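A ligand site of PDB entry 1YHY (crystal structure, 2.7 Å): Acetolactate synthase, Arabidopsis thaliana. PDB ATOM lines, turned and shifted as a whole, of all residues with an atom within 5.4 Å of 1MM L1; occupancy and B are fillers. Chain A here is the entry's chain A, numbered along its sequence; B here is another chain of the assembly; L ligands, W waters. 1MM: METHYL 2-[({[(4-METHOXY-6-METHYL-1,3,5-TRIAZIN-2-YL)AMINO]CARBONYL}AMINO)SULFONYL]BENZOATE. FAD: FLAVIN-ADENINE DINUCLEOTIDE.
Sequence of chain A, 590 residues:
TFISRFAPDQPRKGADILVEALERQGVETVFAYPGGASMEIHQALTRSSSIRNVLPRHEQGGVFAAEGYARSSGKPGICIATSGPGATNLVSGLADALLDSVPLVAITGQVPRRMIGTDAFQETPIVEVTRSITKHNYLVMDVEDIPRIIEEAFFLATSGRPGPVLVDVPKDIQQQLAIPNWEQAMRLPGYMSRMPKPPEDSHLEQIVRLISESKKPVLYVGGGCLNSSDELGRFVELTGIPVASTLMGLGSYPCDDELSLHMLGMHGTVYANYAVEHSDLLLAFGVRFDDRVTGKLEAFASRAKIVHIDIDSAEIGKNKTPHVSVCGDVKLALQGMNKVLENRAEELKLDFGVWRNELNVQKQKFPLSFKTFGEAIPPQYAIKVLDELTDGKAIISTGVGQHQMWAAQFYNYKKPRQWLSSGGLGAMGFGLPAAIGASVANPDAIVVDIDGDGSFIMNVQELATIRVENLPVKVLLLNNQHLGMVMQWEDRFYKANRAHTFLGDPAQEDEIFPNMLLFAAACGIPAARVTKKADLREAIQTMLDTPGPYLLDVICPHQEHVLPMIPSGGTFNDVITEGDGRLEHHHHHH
O9 of 1MM L1 lies within hydrogen-bond range of NH2 of Arg 292, 2.5 Å away. OG of Ser 568 lies within hydrogen-bond range of O7A of 1MM L1 (2.6 Å). NZ of Lys 171 of chain B lies within hydrogen-bond range of N8 of 1MM L1, 3.1 Å away. An oxygen (O4) of FAD L2 sits at hydrogen-bond distance from the backbone NH (N) of Met 266, 3.2 Å away. O4 of FAD L2 is in hydrogen-bond range of N of His 267, at 2.7 Å.
The guanidinium group of Arg 292 lies within salt-bridge range of the side-chain carboxylate of Asp 291. The backbone carbonyl oxygen of Arg 292 sits at hydrogen-bond distance from the backbone NH of Met 266. The side-chain carboxylate (OD1) of Asp 291 is in hydrogen-bond range of the backbone NH (N) of Phe 121 of chain B (3.0 Å). OG1 of Thr 82 of chain B lies within hydrogen-bond range of N of Gly 36 of chain B (3.5 Å). OG1 of Thr 82 of chain B sits at hydrogen-bond distance from N of Ala 37 of chain B (3.0 Å). The side-chain hydroxyl of Ser 83 of chain B sits at hydrogen-bond distance from the backbone carbonyl oxygen of Gln 122 of chain B (2.7 Å).
Residues that only touch 1MM L1: Met 266 (3.8 Å), Asp 291 (3.2 Å), Met 485 (3.8 Å), Val 486 (3.8 Å), Trp 489 (3.3 Å), Gly 36 of chain B (3.3 Å), Ala 37 of chain B (3.4 Å), Val 111 of chain B (3.6 Å), Pro 112 of chain B (3.3 Å), Ala 120 of chain B (3.7 Å), Phe 121 of chain B (3.3 Å) and Gln 122 of chain B (3.5 Å). Within 4 Å of 1MM L1: Met 266, Asp 291, Arg 292, Met 485, Val 486, Trp 489, Ser 568, Gly 36 of chain B, Ala 37 of chain B, Val 111 of chain B, Pro 112 of chain B, Ala 120 of chain B, Phe 121 of chain B, Gln 122 of chain B and Lys 171 of chain B. The nearest printed residue that does not touch 1MM L1 is Met 115 of chain B (4.04 Å).
Water W1 lies within hydrogen-bond range of NE2 of His 267 (2.8 Å), NE1 of Trp 489 (2.9 Å), SD of Met 266 (3.5 Å) and SD of Met 485 (3.7 Å).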
ATOM      1  N   MET A 266       4.569   7.323  12.159  1.00  0.00           N
ATOM      2  CA  MET A 266       3.822   8.370  12.828  1.00  0.00           C
ATOM      3  C   MET A 266       3.856   9.688  12.055  1.00  0.00           C
ATOM      4  O   MET A 266       2.808  10.324  11.873  1.00  0.00           O
ATOM      5  CB  MET A 266       4.369   8.583  14.237  1.00  0.00           C
ATOM      6  CG  MET A 266       3.674   9.672  15.019  1.00  0.00           C
ATOM      7  SD  MET A 266       4.022   9.592  16.790  1.00  0.00           S
ATOM      8  CE  MET A 266       2.880   8.259  17.273  1.00  0.00           C
ATOM      9  N   HIS A 267       5.038  10.082  11.606  1.00  0.00           N
ATOM     10  CA  HIS A 267       5.195  11.311  10.845  1.00  0.00           C
ATOM     11  C   HIS A 267       5.702  11.056   9.444  1.00  0.00           C
ATOM     12  O   HIS A 267       6.344  11.919   8.836  1.00  0.00           O
ATOM     13  CB  HIS A 267       6.119  12.278  11.565  1.00  0.00           C
ATOM     14  CG  HIS A 267       5.525  12.868  12.798  1.00  0.00           C
ATOM     15  ND1 HIS A 267       4.408  13.676  12.771  1.00  0.00           N
ATOM     16  CD2 HIS A 267       5.855  12.748  14.109  1.00  0.00           C
ATOM     17  CE1 HIS A 267       4.084  14.026  14.004  1.00  0.00           C
ATOM     18  NE2 HIS A 267       4.949  13.475  14.830  1.00  0.00           N
ATOM     19  N   ASP A 291       6.757   0.850  17.228  1.00  0.00           N
ATOM     20  CA  ASP A 291       5.395   1.347  17.398  1.00  0.00           C
ATOM     21  C   ASP A 291       5.206   2.712  16.720  1.00  0.00           C
ATOM     22  O   ASP A 291       4.085   3.084  16.376  1.00  0.00           O
ATOM     23  CB  ASP A 291       5.005   1.425  18.878  1.00  0.00           C
ATOM     24  CG  ASP A 291       5.821   2.446  19.654  1.00  0.00           C
ATOM     25  OD1 ASP A 291       6.575   2.059  20.575  1.00  0.00           O
ATOM     26  OD2 ASP A 291       5.692   3.657  19.358  1.00  0.00           O
ATOM     27  N   ARG A 292       6.292   3.442  16.526  1.00  0.00           N
ATOM     28  CA  ARG A 292       6.239   4.732  15.852  1.00  0.00           C
ATOM     29  C   ARG A 292       5.875   4.498  14.387  1.00  0.00           C
ATOM     30  O   ARG A 292       5.179   5.292  13.761  1.00  0.00           O
ATOM     31  CB  ARG A 292       7.598   5.429  15.921  1.00  0.00           C
ATOM     32  CG  ARG A 292       7.718   6.437  17.025  1.00  0.00           C
ATOM     33  CD  ARG A 292       6.870   6.009  18.192  1.00  0.00           C
ATOM     34  NE  ARG A 292       6.099   7.136  18.699  1.00  0.00           N
ATOM     35  CZ  ARG A 292       5.187   7.057  19.654  1.00  0.00           C
ATOM     36  NH1 ARG A 292       4.903   5.890  20.237  1.00  0.00           N
ATOM     37  NH2 ARG A 292       4.587   8.156  20.069  1.00  0.00           N
ATOM     38  N   MET A 485       7.594  19.499  20.182  1.00  0.00           N
ATOM     39  CA  MET A 485       6.788  18.297  20.061  1.00  0.00           C
ATOM     40  C   MET A 485       5.772  18.146  21.197  1.00  0.00           C
ATOM     41  O   MET A 485       4.650  17.688  20.972  1.00  0.00           O
ATOM     42  CB  MET A 485       7.670  17.050  19.977  1.00  0.00           C
ATOM     43  CG  MET A 485       6.914  15.798  19.603  1.00  0.00           C
ATOM     44  SD  MET A 485       5.924  16.002  18.101  1.00  0.00           S
ATOM     45  CE  MET A 485       7.139  15.646  16.857  1.00  0.00           C
ATOM     46  N   VAL A 486       6.157  18.532  22.414  1.00  0.00           N
ATOM     47  CA  VAL A 486       5.219  18.410  23.517  1.00  0.00           C
ATOM     48  C   VAL A 486       4.102  19.443  23.426  1.00  0.00           C
ATOM     49  O   VAL A 486       2.966  19.151  23.793  1.00  0.00           O
ATOM     50  CB  VAL A 486       5.929  18.553  24.878  1.00  0.00           C
ATOM     51  CG1 VAL A 486       4.922  18.371  25.997  1.00  0.00           C
ATOM     52  CG2 VAL A 486       7.003  17.501  24.998  1.00  0.00           C
ATOM     53  N   TRP A 489       1.360  18.233  21.032  1.00  0.00           N
ATOM     54  CA  TRP A 489       0.428  17.312  21.641  1.00  0.00           C
ATOM     55  C   TRP A 489      -0.520  18.059  22.575  1.00  0.00           C
ATOM     56  O   TRP A 489      -1.663  17.648  22.757  1.00  0.00           O
ATOM     57  CB  TRP A 489       1.174  16.207  22.388  1.00  0.00           C
ATOM     58  CG  TRP A 489       1.676  15.119  21.475  1.00  0.00           C
ATOM     59  CD1 TRP A 489       2.448  15.271  20.366  1.00  0.00           C
ATOM     60  CD2 TRP A 489       1.383  13.720  21.576  1.00  0.00           C
ATOM     61  NE1 TRP A 489       2.655  14.057  19.752  1.00  0.00           N
ATOM     62  CE2 TRP A 489       2.009  13.089  20.482  1.00  0.00           C
ATOM     63  CE3 TRP A 489       0.660  12.942  22.482  1.00  0.00           C
ATOM     64  CZ2 TRP A 489       1.934  11.706  20.271  1.00  0.00           C
ATOM     65  CZ3 TRP A 489       0.580  11.568  22.280  1.00  0.00           C
ATOM     66  CH2 TRP A 489       1.218  10.964  21.176  1.00  0.00           C
ATOM     67  N   SER A 568      -0.655   8.117  18.157  1.00  0.00           N
ATOM     68  CA  SER A 568      -0.057   6.918  18.749  1.00  0.00           C
ATOM     69  C   SER A 568      -1.044   5.768  18.804  1.00  0.00           C
ATOM     70  O   SER A 568      -2.122   5.907  19.374  1.00  0.00           O
ATOM     71  CB  SER A 568       0.469   7.228  20.142  1.00  0.00           C
ATOM     72  OG  SER A 568       1.171   6.116  20.668  1.00  0.00           O
ATOM     73  N   GLY B  35       7.717  15.605  29.350  1.00  0.00           N
ATOM     74  CA  GLY B  35       8.079  14.661  28.309  1.00  0.00           C
ATOM     75  C   GLY B  35       6.826  13.909  27.905  1.00  0.00           C
ATOM     76  O   GLY B  35       5.805  13.978  28.602  1.00  0.00           O
ATOM     77  N   GLY B  36       6.876  13.167  26.801  1.00  0.00           N
ATOM     78  CA  GLY B  36       5.713  12.430  26.332  1.00  0.00           C
ATOM     79  C   GLY B  36       4.991  11.568  27.354  1.00  0.00           C
ATOM     80  O   GLY B  36       3.777  11.668  27.514  1.00  0.00           O
ATOM     81  N   ALA B  37       5.744  10.722  28.059  1.00  0.00           N
ATOM     82  CA  ALA B  37       5.167   9.813  29.045  1.00  0.00           C
ATOM     83  C   ALA B  37       4.671  10.471  30.327  1.00  0.00           C
ATOM     84  O   ALA B  37       4.001   9.835  31.128  1.00  0.00           O
ATOM     85  CB  ALA B  37       6.172   8.721  29.380  1.00  0.00           C
ATOM     86  N   MET B  39       3.159  13.800  30.237  1.00  0.00           N
ATOM     87  CA  MET B  39       2.276  14.918  29.910  1.00  0.00           C
ATOM     88  C   MET B  39       1.076  15.020  30.831  1.00  0.00           C
ATOM     89  O   MET B  39       0.739  16.114  31.300  1.00  0.00           O
ATOM     90  CB  MET B  39       1.785  14.810  28.468  1.00  0.00           C
ATOM     91  CG  MET B  39       2.835  15.159  27.437  1.00  0.00           C
ATOM     92  SD  MET B  39       2.087  15.411  25.833  1.00  0.00           S
ATOM     93  CE  MET B  39       1.545  17.127  25.987  1.00  0.00           C
ATOM     94  N   THR B  82      10.117  12.464  32.468  1.00  0.00           N
ATOM     95  CA  THR B  82       9.386  11.575  31.568  1.00  0.00           C
ATOM     96  C   THR B  82      10.141  10.241  31.460  1.00  0.00           C
ATOM     97  O   THR B  82      11.120  10.013  32.163  1.00  0.00           O
ATOM     98  CB  THR B  82       9.231  12.211  30.165  1.00  0.00           C
ATOM     99  OG1 THR B  82       8.412  11.367  29.339  1.00  0.00           O
ATOM    100  CG2 THR B  82      10.581  12.370  29.500  1.00  0.00           C
ATOM    101  N   SER B  83       9.691   9.354  30.576  1.00  0.00           N
ATOM    102  CA  SER B  83      10.330   8.062  30.432  1.00  0.00           C
ATOM    103  C   SER B  83      11.637   8.158  29.656  1.00  0.00           C
ATOM    104  O   SER B  83      12.070   9.253  29.299  1.00  0.00           O
ATOM    105  CB  SER B  83       9.392   7.094  29.716  1.00  0.00           C
ATOM    106  OG  SER B  83       9.072   7.558  28.418  1.00  0.00           O
ATOM    107  N   GLN B 110       6.311   6.465  32.323  1.00  0.00           N
ATOM    108  CA  GLN B 110       6.676   5.201  31.690  1.00  0.00           C
ATOM    109  C   GLN B 110       5.712   4.982  30.549  1.00  0.00           C
ATOM    110  O   GLN B 110       4.628   5.547  30.525  1.00  0.00           O
ATOM    111  CB  GLN B 110       6.525   4.028  32.651  1.00  0.00           C
ATOM    112  CG  GLN B 110       7.808   3.277  32.956  1.00  0.00           C
ATOM    113  CD  GLN B 110       8.545   2.779  31.730  1.00  0.00           C
ATOM    114  OE1 GLN B 110       9.652   2.243  31.847  1.00  0.00           O
ATOM    115  NE2 GLN B 110       7.949   2.938  30.562  1.00  0.00           N
ATOM    116  N   VAL B 111       6.121   4.149  29.607  1.00  0.00           N
ATOM    117  CA  VAL B 111       5.268   3.828  28.485  1.00  0.00           C
ATOM    118  C   VAL B 111       4.099   3.037  29.077  1.00  0.00           C
ATOM    119  O   VAL B 111       4.177   2.567  30.229  1.00  0.00           O
ATOM    120  CB  VAL B 111       6.038   2.976  27.461  1.00  0.00           C
ATOM    121  CG1 VAL B 111       7.302   3.719  27.022  1.00  0.00           C
ATOM    122  CG2 VAL B 111       6.416   1.631  28.062  1.00  0.00           C
ATOM    123  N   PRO B 112       2.986   2.893  28.344  1.00  0.00           N
ATOM    124  CA  PRO B 112       1.852   2.131  28.886  1.00  0.00           C
ATOM    125  C   PRO B 112       2.290   0.711  29.280  1.00  0.00           C
ATOM    126  O   PRO B 112       3.211   0.147  28.677  1.00  0.00           O
ATOM    127  CB  PRO B 112       0.860   2.133  27.734  1.00  0.00           C
ATOM    128  CG  PRO B 112       1.137   3.448  27.065  1.00  0.00           C
ATOM    129  CD  PRO B 112       2.653   3.477  27.033  1.00  0.00           C
ATOM    130  N   MET B 115       3.077  -2.046  26.831  1.00  0.00           N
ATOM    131  CA  MET B 115       4.236  -1.764  25.995  1.00  0.00           C
ATOM    132  C   MET B 115       5.557  -2.053  26.695  1.00  0.00           C
ATOM    133  O   MET B 115       6.614  -2.076  26.062  1.00  0.00           O
ATOM    134  CB  MET B 115       4.226  -0.286  25.587  1.00  0.00           C
ATOM    135  CG  MET B 115       3.015   0.145  24.795  1.00  0.00           C
ATOM    136  SD  MET B 115       3.099  -0.517  23.164  1.00  0.00           S
ATOM    137  CE  MET B 115       1.353  -0.669  22.793  1.00  0.00           C
ATOM    138  N   ALA B 120       9.712  -0.290  23.437  1.00  0.00           N
ATOM    139  CA  ALA B 120       8.847   0.788  22.984  1.00  0.00           C
ATOM    140  C   ALA B 120       9.561   2.135  22.896  1.00  0.00           C
ATOM    141  O   ALA B 120      10.686   2.294  23.352  1.00  0.00           O
ATOM    142  CB  ALA B 120       7.632   0.903  23.906  1.00  0.00           C
ATOM    143  N   PHE B 121       8.872   3.094  22.294  1.00  0.00           N
ATOM    144  CA  PHE B 121       9.379   4.449  22.144  1.00  0.00           C
ATOM    145  C   PHE B 121       9.692   5.048  23.508  1.00  0.00           C
ATOM    146  O   PHE B 121       8.836   5.063  24.411  1.00  0.00           O
ATOM    147  CB  PHE B 121       8.323   5.282  21.422  1.00  0.00           C
ATOM    148  CG  PHE B 121       8.719   6.701  21.207  1.00  0.00           C
ATOM    149  CD1 PHE B 121       9.860   7.026  20.475  1.00  0.00           C
ATOM    150  CD2 PHE B 121       7.948   7.739  21.735  1.00  0.00           C
ATOM    151  CE1 PHE B 121      10.210   8.351  20.276  1.00  0.00           C
ATOM    152  CE2 PHE B 121       8.298   9.064  21.536  1.00  0.00           C
ATOM    153  CZ  PHE B 121       9.437   9.372  20.797  1.00  0.00           C
ATOM    154  N   GLN B 122      10.911   5.544  23.669  1.00  0.00           N
ATOM    155  CA  GLN B 122      11.347   6.170  24.911  1.00  0.00           C
ATOM    156  C   GLN B 122      11.117   5.279  26.134  1.00  0.00           C
ATOM    157  O   GLN B 122      10.626   5.739  27.158  1.00  0.00           O
ATOM    158  CB  GLN B 122      10.656   7.517  25.124  1.00  0.00           C
ATOM    159  CG  GLN B 122      10.717   8.433  23.908  1.00  0.00           C
ATOM    160  CD  GLN B 122      10.620   9.908  24.273  1.00  0.00           C
ATOM    161  OE1 GLN B 122      11.623  10.631  24.281  1.00  0.00           O
ATOM    162  NE2 GLN B 122       9.404  10.353  24.591  1.00  0.00           N
ATOM    163  N   LYS B 171       1.999   5.538  31.608  1.00  0.00           N
ATOM    164  CA  LYS B 171       1.082   6.525  31.085  1.00  0.00           C
ATOM    165  C   LYS B 171      -0.376   6.106  31.102  1.00  0.00           C
ATOM    166  O   LYS B 171      -1.257   6.927  31.361  1.00  0.00           O
ATOM    167  CB  LYS B 171       1.465   6.915  29.660  1.00  0.00           C
ATOM    168  CG  LYS B 171       0.484   7.889  29.031  1.00  0.00           C
ATOM    169  CD  LYS B 171       0.993   8.473  27.724  1.00  0.00           C
ATOM    170  CE  LYS B 171      -0.056   9.373  27.113  1.00  0.00           C
ATOM    171  NZ  LYS B 171       0.438  10.061  25.895  1.00  0.00           N
HETATM  172  C4  1MM L   1       3.751   3.446  22.581  1.00  0.00           C
HETATM  173  C5  1MM L   1       5.117   3.468  23.021  1.00  0.00           C
HETATM  174  C6  1MM L   1       5.577   4.492  23.935  1.00  0.00           C
HETATM  175  C1  1MM L   1       4.659   5.538  24.423  1.00  0.00           C
HETATM  176  C2  1MM L   1       3.269   5.509  23.960  1.00  0.00           C
HETATM  177  C3  1MM L   1       2.775   4.466  23.030  1.00  0.00           C
HETATM  178  S7  1MM L   1       1.820   6.569  24.285  1.00  0.00           S
HETATM  179  N8  1MM L   1       2.383   8.164  24.330  1.00  0.00           N
HETATM  180  C9  1MM L   1       3.071   8.728  23.313  1.00  0.00           C
HETATM  181  N10 1MM L   1       3.357   9.970  23.640  1.00  0.00           N
HETATM  182  C2' 1MM L   1       4.038  10.869  22.946  1.00  0.00           C
HETATM  183  N1' 1MM L   1       4.216  12.211  23.446  1.00  0.00           N
HETATM  184  C6' 1MM L   1       4.960  13.212  22.697  1.00  0.00           C
HETATM  185  N5' 1MM L   1       5.531  12.833  21.443  1.00  0.00           N
HETATM  186  C4' 1MM L   1       5.354  11.477  20.946  1.00  0.00           C
HETATM  187  N3' 1MM L   1       4.623  10.520  21.692  1.00  0.00           N
HETATM  188  O7A 1MM L   1       0.900   6.598  23.168  1.00  0.00           O
HETATM  189  O7B 1MM L   1       1.231   6.412  25.584  1.00  0.00           O
HETATM  190  O9  1MM L   1       3.354   8.066  22.264  1.00  0.00           O
HETATM  191  C11 1MM L   1       5.014   6.677  25.409  1.00  0.00           C
HETATM  192  O12 1MM L   1       5.970   7.515  24.736  1.00  0.00           O
HETATM  193  C13 1MM L   1       6.463   8.658  25.416  1.00  0.00           C
HETATM  194  O11 1MM L   1       4.489   6.782  26.549  1.00  0.00           O
HETATM  195  O4' 1MM L   1       5.912  11.123  19.746  1.00  0.00           O
HETATM  196  C5' 1MM L   1       6.678  11.753  18.742  1.00  0.00           C
HETATM  197  C7' 1MM L   1       5.162  14.637  23.202  1.00  0.00           C
HETATM  198  PA  FAD L   2      16.817   0.276  14.193  1.00  0.00           P
HETATM  199  O1A FAD L   2      18.205   0.767  14.031  1.00  0.00           O
HETATM  200  O2A FAD L   2      16.061   0.597  15.380  1.00  0.00           O
HETATM  201  O5B FAD L   2      16.709  -1.212  14.082  1.00  0.00           O
HETATM  202  C5B FAD L   2      17.455  -1.893  13.014  1.00  0.00           C
HETATM  203  C4B FAD L   2      17.079  -3.358  13.040  1.00  0.00           C
HETATM  204  O4B FAD L   2      17.873  -3.935  12.007  1.00  0.00           O
HETATM  205  C3B FAD L   2      17.305  -4.325  14.292  1.00  0.00           C
HETATM  206  O3B FAD L   2      16.253  -5.230  14.538  1.00  0.00           O
HETATM  207  C2B FAD L   2      18.632  -4.903  13.991  1.00  0.00           C
HETATM  208  O2B FAD L   2      19.180  -5.874  14.793  1.00  0.00           O
HETATM  209  C1B FAD L   2      18.491  -5.114  12.480  1.00  0.00           C
HETATM  210  N9A FAD L   2      19.800  -5.204  11.682  1.00  0.00           N
HETATM  211  C8A FAD L   2      20.977  -4.429  12.083  1.00  0.00           C
HETATM  212  N7A FAD L   2      22.036  -4.584  11.340  1.00  0.00           N
HETATM  213  C5A FAD L   2      21.664  -5.483  10.400  1.00  0.00           C
HETATM  214  C6A FAD L   2      22.289  -6.201   9.166  1.00  0.00           C
HETATM  215  N6A FAD L   2      23.542  -5.962   8.816  1.00  0.00           N
HETATM  216  N1A FAD L   2      21.487  -7.135   8.387  1.00  0.00           N
HETATM  217  C2A FAD L   2      20.104  -7.426   8.749  1.00  0.00           C
HETATM  218  N3A FAD L   2      19.451  -6.836   9.828  1.00  0.00           N
HETATM  219  C4A FAD L   2      20.244  -5.870  10.624  1.00  0.00           C
HETATM  220  N1  FAD L   2      10.545   6.380  12.959  1.00  0.00           N
HETATM  221  C2  FAD L   2       9.858   6.249  11.825  1.00  0.00           C
HETATM  222  O2  FAD L   2      10.265   5.414  11.013  1.00  0.00           O
HETATM  223  N3  FAD L   2       8.766   7.086  11.513  1.00  0.00           N
HETATM  224  C4  FAD L   2       8.364   8.140  12.369  1.00  0.00           C
HETATM  225  O4  FAD L   2       7.347   8.813  12.146  1.00  0.00           O
HETATM  226  C4X FAD L   2       9.177   8.353  13.572  1.00  0.00           C
HETATM  227  N5  FAD L   2       8.869   9.405  14.419  1.00  0.00           N
HETATM  228  C5X FAD L   2       9.662   9.605  15.535  1.00  0.00           C
HETATM  229  C6  FAD L   2       9.443  10.806  16.296  1.00  0.00           C
HETATM  230  C7  FAD L   2      10.341  11.167  17.350  1.00  0.00           C
HETATM  231  C7M FAD L   2      10.166  12.514  17.998  1.00  0.00           C
HETATM  232  C8  FAD L   2      11.456  10.280  17.688  1.00  0.00           C
HETATM  233  C8M FAD L   2      12.517  10.656  18.717  1.00  0.00           C
HETATM  234  C9  FAD L   2      11.620   9.044  16.985  1.00  0.00           C
HETATM  235  C9A FAD L   2      10.789   8.701  15.861  1.00  0.00           C
HETATM  236  N10 FAD L   2      10.983   7.554  15.053  1.00  0.00           N
HETATM  237  C10 FAD L   2      10.258   7.406  13.848  1.00  0.00           C
HETATM  238  C1' FAD L   2      12.205   6.694  15.241  1.00  0.00           C
HETATM  239  C2' FAD L   2      11.697   5.484  15.908  1.00  0.00           C
HETATM  240  O2' FAD L   2      11.589   5.634  17.320  1.00  0.00           O
HETATM  241  C3' FAD L   2      12.536   4.203  15.716  1.00  0.00           C
HETATM  242  O3' FAD L   2      13.944   4.585  16.199  1.00  0.00           O
HETATM  243  C4' FAD L   2      12.769   3.740  14.249  1.00  0.00           C
HETATM  244  O4' FAD L   2      11.391   3.534  13.661  1.00  0.00           O
HETATM  245  C5' FAD L   2      13.523   2.477  14.275  1.00  0.00           C
HETATM  246  O5' FAD L   2      13.678   2.053  12.889  1.00  0.00           O
HETATM  247  P   FAD L   2      14.448   0.747  12.532  1.00  0.00           P
HETATM  248  O1P FAD L   2      13.755  -0.342  13.253  1.00  0.00           O
HETATM  249  O2P FAD L   2      14.370   0.649  11.125  1.00  0.00           O
HETATM  250  O3P FAD L   2      15.991   0.871  12.945  1.00  0.00           O
HETATM  251  O   HOH W   1       3.966  12.987  17.457  1.00  0.00           O
HETATM  252  O   HOH W   2       2.432  11.897  25.185  1.00  0.00           O
